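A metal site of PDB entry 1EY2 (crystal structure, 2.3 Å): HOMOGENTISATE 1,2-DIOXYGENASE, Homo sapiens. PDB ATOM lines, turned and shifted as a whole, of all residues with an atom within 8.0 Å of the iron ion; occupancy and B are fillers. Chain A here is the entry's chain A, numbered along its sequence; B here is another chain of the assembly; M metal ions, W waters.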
ATOM      1  N   PRO A 321       0.954  -7.168   9.056  1.00  0.00           N
ATOM      2  CA  PRO A 321      -0.064  -8.034   8.461  1.00  0.00           C
ATOM      3  C   PRO A 321       0.214  -9.514   8.278  1.00  0.00           C
ATOM      4  O   PRO A 321      -0.697 -10.297   8.064  1.00  0.00           O
ATOM      5  CB  PRO A 321      -0.395  -7.314   7.138  1.00  0.00           C
ATOM      6  CG  PRO A 321       0.872  -6.669   6.768  1.00  0.00           C
ATOM      7  CD  PRO A 321       1.397  -6.145   8.096  1.00  0.00           C
ATOM      8  N   PRO A 358      -3.424   0.950   9.089  1.00  0.00           N
ATOM      9  CA  PRO A 358      -2.156   0.462   8.547  1.00  0.00           C
ATOM     10  C   PRO A 358      -1.130   1.612   8.517  1.00  0.00           C
ATOM     11  O   PRO A 358      -1.492   2.752   8.212  1.00  0.00           O
ATOM     12  CB  PRO A 358      -2.530   0.067   7.115  1.00  0.00           C
ATOM     13  CG  PRO A 358      -3.937  -0.357   7.231  1.00  0.00           C
ATOM     14  CD  PRO A 358      -4.531   0.685   8.146  1.00  0.00           C
ATOM     15  N   TYR A 359       0.109   1.329   8.874  1.00  0.00           N
ATOM     16  CA  TYR A 359       1.172   2.322   8.840  1.00  0.00           C
ATOM     17  C   TYR A 359       1.593   2.628   7.395  1.00  0.00           C
ATOM     18  O   TYR A 359       1.261   1.841   6.501  1.00  0.00           O
ATOM     19  CB  TYR A 359       2.371   1.782   9.610  1.00  0.00           C
ATOM     20  CG  TYR A 359       2.692   0.313   9.345  1.00  0.00           C
ATOM     21  CD1 TYR A 359       3.288  -0.090   8.142  1.00  0.00           C
ATOM     22  CD2 TYR A 359       2.431  -0.670  10.312  1.00  0.00           C
ATOM     23  CE1 TYR A 359       3.634  -1.421   7.926  1.00  0.00           C
ATOM     24  CE2 TYR A 359       2.757  -1.999  10.101  1.00  0.00           C
ATOM     25  CZ  TYR A 359       3.360  -2.364   8.911  1.00  0.00           C
ATOM     26  OH  TYR A 359       3.688  -3.683   8.704  1.00  0.00           O
ATOM     27  N   TYR A 360       2.259   3.759   7.141  1.00  0.00           N
ATOM     28  CA  TYR A 360       2.784   4.034   5.792  1.00  0.00           C
ATOM     29  C   TYR A 360       3.857   2.976   5.532  1.00  0.00           C
ATOM     30  O   TYR A 360       4.595   2.625   6.458  1.00  0.00           O
ATOM     31  CB  TYR A 360       3.294   5.469   5.672  1.00  0.00           C
ATOM     32  CG  TYR A 360       2.140   6.444   5.688  1.00  0.00           C
ATOM     33  CD1 TYR A 360       1.691   7.005   6.887  1.00  0.00           C
ATOM     34  CD2 TYR A 360       1.426   6.717   4.517  1.00  0.00           C
ATOM     35  CE1 TYR A 360       0.557   7.810   6.919  1.00  0.00           C
ATOM     36  CE2 TYR A 360       0.290   7.525   4.540  1.00  0.00           C
ATOM     37  CZ  TYR A 360      -0.149   8.059   5.749  1.00  0.00           C
ATOM     38  OH  TYR A 360      -1.295   8.833   5.783  1.00  0.00           O
ATOM     39  N   HIS A 361       4.007   2.537   4.294  1.00  0.00           N
ATOM     40  CA  HIS A 361       4.859   1.395   4.049  1.00  0.00           C
ATOM     41  C   HIS A 361       5.449   1.362   2.653  1.00  0.00           C
ATOM     42  O   HIS A 361       4.839   1.808   1.669  1.00  0.00           O
ATOM     43  CB  HIS A 361       3.943   0.151   4.259  1.00  0.00           C
ATOM     44  CG  HIS A 361       4.625  -1.183   4.340  1.00  0.00           C
ATOM     45  ND1 HIS A 361       4.004  -2.330   3.853  1.00  0.00           N
ATOM     46  CD2 HIS A 361       5.766  -1.618   4.934  1.00  0.00           C
ATOM     47  CE1 HIS A 361       4.733  -3.380   4.144  1.00  0.00           C
ATOM     48  NE2 HIS A 361       5.805  -2.994   4.791  1.00  0.00           N
ATOM     49  N   ARG A 362       6.689   0.878   2.602  1.00  0.00           N
ATOM     50  CA  ARG A 362       7.403   0.605   1.369  1.00  0.00           C
ATOM     51  C   ARG A 362       7.891  -0.833   1.660  1.00  0.00           C
ATOM     52  O   ARG A 362       8.558  -1.088   2.684  1.00  0.00           O
ATOM     53  CB  ARG A 362       8.533   1.597   1.154  1.00  0.00           C
ATOM     54  CG  ARG A 362       7.992   2.945   0.686  1.00  0.00           C
ATOM     55  CD  ARG A 362       8.819   4.068   1.259  1.00  0.00           C
ATOM     56  NE  ARG A 362      10.203   3.995   0.822  1.00  0.00           N
ATOM     57  CZ  ARG A 362      11.222   4.610   1.428  1.00  0.00           C
ATOM     58  NH1 ARG A 362      11.009   5.339   2.519  1.00  0.00           N
ATOM     59  NH2 ARG A 362      12.447   4.506   0.948  1.00  0.00           N
ATOM     60  N   ASN A 363       7.584  -1.746   0.745  1.00  0.00           N
ATOM     61  CA  ASN A 363       7.852  -3.168   0.982  1.00  0.00           C
ATOM     62  C   ASN A 363       8.584  -3.852  -0.164  1.00  0.00           C
ATOM     63  O   ASN A 363       8.339  -3.544  -1.339  1.00  0.00           O
ATOM     64  CB  ASN A 363       6.476  -3.853   1.185  1.00  0.00           C
ATOM     65  CG  ASN A 363       6.563  -5.245   1.793  1.00  0.00           C
ATOM     66  OD1 ASN A 363       7.628  -5.766   2.119  1.00  0.00           O
ATOM     67  ND2 ASN A 363       5.394  -5.829   2.001  1.00  0.00           N
ATOM     68  N   MET A 365       8.080  -6.812  -1.028  1.00  0.00           N
ATOM     69  CA  MET A 365       7.151  -7.776  -1.605  1.00  0.00           C
ATOM     70  C   MET A 365       6.065  -7.073  -2.435  1.00  0.00           C
ATOM     71  O   MET A 365       5.824  -5.892  -2.246  1.00  0.00           O
ATOM     72  CB  MET A 365       6.446  -8.580  -0.490  1.00  0.00           C
ATOM     73  CG  MET A 365       7.294  -8.995   0.683  1.00  0.00           C
ATOM     74  SD  MET A 365       8.467 -10.399   0.406  1.00  0.00           S
ATOM     75  CE  MET A 365       7.292 -11.784   0.663  1.00  0.00           C
ATOM     76  N   SER A 366       5.490  -7.762  -3.422  1.00  0.00           N
ATOM     77  CA  SER A 366       4.359  -7.206  -4.179  1.00  0.00           C
ATOM     78  C   SER A 366       3.111  -7.509  -3.328  1.00  0.00           C
ATOM     79  O   SER A 366       3.046  -8.547  -2.667  1.00  0.00           O
ATOM     80  CB  SER A 366       4.180  -7.895  -5.519  1.00  0.00           C
ATOM     81  OG  SER A 366       5.400  -8.045  -6.202  1.00  0.00           O
ATOM     82  N   GLU A 367       2.115  -6.611  -3.355  1.00  0.00           N
ATOM     83  CA  GLU A 367       0.912  -6.824  -2.566  1.00  0.00           C
ATOM     84  C   GLU A 367      -0.350  -6.715  -3.392  1.00  0.00           C
ATOM     85  O   GLU A 367      -0.638  -5.631  -3.912  1.00  0.00           O
ATOM     86  CB  GLU A 367       0.817  -5.809  -1.432  1.00  0.00           C
ATOM     87  CG  GLU A 367       1.955  -5.828  -0.432  1.00  0.00           C
ATOM     88  CD  GLU A 367       1.926  -4.620   0.488  1.00  0.00           C
ATOM     89  OE1 GLU A 367       0.874  -3.951   0.559  1.00  0.00           O
ATOM     90  OE2 GLU A 367       2.958  -4.309   1.125  1.00  0.00           O
ATOM     91  N   MET A 369      -4.367  -7.091  -3.365  1.00  0.00           N
ATOM     92  CA  MET A 369      -5.432  -7.024  -2.375  1.00  0.00           C
ATOM     93  C   MET A 369      -6.783  -7.260  -3.032  1.00  0.00           C
ATOM     94  O   MET A 369      -7.050  -6.742  -4.119  1.00  0.00           O
ATOM     95  CB  MET A 369      -5.395  -5.641  -1.741  1.00  0.00           C
ATOM     96  CG  MET A 369      -5.959  -5.560  -0.343  1.00  0.00           C
ATOM     97  SD  MET A 369      -4.675  -5.274   0.876  1.00  0.00           S
ATOM     98  CE  MET A 369      -5.655  -4.948   2.310  1.00  0.00           C
ATOM     99  N   HIS A 391      -0.089  -3.068  -5.146  1.00  0.00           N
ATOM    100  CA  HIS A 391       0.985  -2.216  -4.690  1.00  0.00           C
ATOM    101  C   HIS A 391       2.255  -2.942  -5.106  1.00  0.00           C
ATOM    102  O   HIS A 391       2.590  -3.988  -4.538  1.00  0.00           O
ATOM    103  CB  HIS A 391       0.984  -2.070  -3.183  1.00  0.00           C
ATOM    104  CG  HIS A 391      -0.214  -1.357  -2.645  1.00  0.00           C
ATOM    105  ND1 HIS A 391      -0.717  -1.606  -1.379  1.00  0.00           N
ATOM    106  CD2 HIS A 391      -1.005  -0.403  -3.180  1.00  0.00           C
ATOM    107  CE1 HIS A 391      -1.764  -0.817  -1.164  1.00  0.00           C
ATOM    108  NE2 HIS A 391      -1.959  -0.087  -2.249  1.00  0.00           N
ATOM    109  N   THR A 395       6.987   0.650  -3.942  1.00  0.00           N
ATOM    110  CA  THR A 395       6.168   1.811  -4.257  1.00  0.00           C
ATOM    111  C   THR A 395       5.484   2.165  -2.933  1.00  0.00           C
ATOM    112  O   THR A 395       4.870   1.306  -2.288  1.00  0.00           O
ATOM    113  CB  THR A 395       5.117   1.470  -5.319  1.00  0.00           C
ATOM    114  OG1 THR A 395       5.765   1.082  -6.528  1.00  0.00           O
ATOM    115  CG2 THR A 395       4.246   2.687  -5.612  1.00  0.00           C
ATOM    116  N   PRO A 396       5.595   3.444  -2.499  1.00  0.00           N
ATOM    117  CA  PRO A 396       5.011   3.882  -1.219  1.00  0.00           C
ATOM    118  C   PRO A 396       3.509   3.685  -1.147  1.00  0.00           C
ATOM    119  O   PRO A 396       2.819   3.836  -2.140  1.00  0.00           O
ATOM    120  CB  PRO A 396       5.309   5.376  -1.215  1.00  0.00           C
ATOM    121  CG  PRO A 396       6.521   5.501  -2.063  1.00  0.00           C
ATOM    122  CD  PRO A 396       6.218   4.581  -3.202  1.00  0.00           C
ATOM    123  N   HIS A 397       3.011   3.307   0.023  1.00  0.00           N
ATOM    124  CA  HIS A 397       1.566   3.178   0.209  1.00  0.00           C
ATOM    125  C   HIS A 397       1.272   3.423   1.677  1.00  0.00           C
ATOM    126  O   HIS A 397       2.192   3.559   2.501  1.00  0.00           O
ATOM    127  CB  HIS A 397       1.004   1.848  -0.309  1.00  0.00           C
ATOM    128  CG  HIS A 397       1.713   0.626   0.205  1.00  0.00           C
ATOM    129  ND1 HIS A 397       2.892   0.175  -0.336  1.00  0.00           N
ATOM    130  CD2 HIS A 397       1.385  -0.246   1.197  1.00  0.00           C
ATOM    131  CE1 HIS A 397       3.267  -0.929   0.288  1.00  0.00           C
ATOM    132  NE2 HIS A 397       2.381  -1.214   1.209  1.00  0.00           N
ATOM    133  N   GLY A 398      -0.012   3.561   1.997  1.00  0.00           N
ATOM    134  CA  GLY A 398      -0.419   3.825   3.377  1.00  0.00           C
ATOM    135  C   GLY A 398      -1.778   4.483   3.391  1.00  0.00           C
ATOM    136  O   GLY A 398      -2.355   4.727   2.321  1.00  0.00           O
ATOM    137  N   MET A 425      -5.143 -10.550   1.103  1.00  0.00           N
ATOM    138  CA  MET A 425      -3.974 -10.197   0.332  1.00  0.00           C
ATOM    139  C   MET A 425      -3.201 -11.425  -0.148  1.00  0.00           C
ATOM    140  O   MET A 425      -3.086 -12.437   0.559  1.00  0.00           O
ATOM    141  CB  MET A 425      -3.034  -9.298   1.177  1.00  0.00           C
ATOM    142  CG  MET A 425      -1.672  -9.014   0.533  1.00  0.00           C
ATOM    143  SD  MET A 425      -0.493  -7.959   1.485  1.00  0.00           S
ATOM    144  CE  MET A 425      -0.063  -8.932   2.960  1.00  0.00           C
ATOM    145  N   GLU A 427       0.352 -11.849  -1.177  1.00  0.00           N
ATOM    146  CA  GLU A 427       1.622 -11.150  -1.275  1.00  0.00           C
ATOM    147  C   GLU A 427       2.723 -12.093  -1.749  1.00  0.00           C
ATOM    148  O   GLU A 427       2.766 -13.254  -1.348  1.00  0.00           O
ATOM    149  CB  GLU A 427       2.010 -10.428   0.020  1.00  0.00           C
ATOM    150  CG  GLU A 427       2.658 -11.207   1.105  1.00  0.00           C
ATOM    151  CD  GLU A 427       3.375 -10.323   2.137  1.00  0.00           C
ATOM    152  OE1 GLU A 427       3.805  -9.199   1.813  1.00  0.00           O
ATOM    153  OE2 GLU A 427       3.500 -10.774   3.292  1.00  0.00           O
ATOM    154  N   GLN B  69       7.244   2.560   7.583  1.00  0.00           N
ATOM    155  CA  GLN B  69       8.118   1.392   7.675  1.00  0.00           C
ATOM    156  C   GLN B  69       8.654   0.979   6.317  1.00  0.00           C
ATOM    157  O   GLN B  69       7.908   0.932   5.335  1.00  0.00           O
ATOM    158  CB  GLN B  69       7.438   0.182   8.340  1.00  0.00           C
ATOM    159  CG  GLN B  69       8.407  -0.994   8.560  1.00  0.00           C
ATOM    160  CD  GLN B  69       7.818  -2.170   9.328  1.00  0.00           C
ATOM    161  OE1 GLN B  69       8.539  -2.893  10.035  1.00  0.00           O
ATOM    162  NE2 GLN B  69       6.540  -2.400   9.195  1.00  0.00           N
ATOM    163  N   SER B  71      10.394  -2.076   4.705  1.00  0.00           N
ATOM    164  CA  SER B  71      10.677  -3.493   4.919  1.00  0.00           C
ATOM    165  C   SER B  71      11.683  -4.011   3.897  1.00  0.00           C
ATOM    166  O   SER B  71      11.401  -4.030   2.690  1.00  0.00           O
ATOM    167  CB  SER B  71       9.398  -4.304   4.820  1.00  0.00           C
ATOM    168  OG  SER B  71       8.386  -3.797   5.664  1.00  0.00           O
ATOM    169  N   PHE B  75       8.257 -10.249   6.154  1.00  0.00           N
ATOM    170  CA  PHE B  75       7.966 -10.099   7.584  1.00  0.00           C
ATOM    171  C   PHE B  75       8.305 -11.338   8.393  1.00  0.00           C
ATOM    172  O   PHE B  75       8.679 -11.238   9.567  1.00  0.00           O
ATOM    173  CB  PHE B  75       6.479  -9.812   7.832  1.00  0.00           C
ATOM    174  CG  PHE B  75       6.017  -8.457   7.426  1.00  0.00           C
ATOM    175  CD1 PHE B  75       5.021  -8.312   6.454  1.00  0.00           C
ATOM    176  CD2 PHE B  75       6.517  -7.314   8.048  1.00  0.00           C
ATOM    177  CE1 PHE B  75       4.538  -7.042   6.118  1.00  0.00           C
ATOM    178  CE2 PHE B  75       6.033  -6.044   7.712  1.00  0.00           C
ATOM    179  CZ  PHE B  75       5.038  -5.913   6.746  1.00  0.00           C
HETATM  180 FE    FE M   1       1.942  -2.889   2.767  1.00  0.00          FE
HETATM  181  O   HOH W   1      -0.495  -2.642   3.640  1.00  0.00           O
HETATM  182  O   HOH W   2       1.867  -4.016   4.262  1.00  0.00           O
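ND1 of His 397 lies within hydrogen-bond range of O of Thr 395.
The side-chain hydroxyl of Ser 71 of chain B is in hydrogen-bond range of a ring nitrogen (NE2) of His 361 (2.8 Å).
N of His 391 sits at hydrogen-bond distance from O of Glu 367, 2.9 Å away.
OE2 of Glu 367 sits close to ND2 of Asn 363 (3.0 Å).
Of the 21 residues printed, 3 come within 4 Å of the iron ion.
Along chain A the residues within 4 Å of the iron ion span positions 361 to 397.
The iron ion is bound by water W2 (1.9 Å), NE2 of His 397 (2.3 Å), ND1 of His 361 (2.4 Å), OE2 of Glu 367 (2.4 Å) and water W1 (2.6 Å).
Slightly farther from the iron ion lies OE1 of Glu 367 (2.7 Å).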
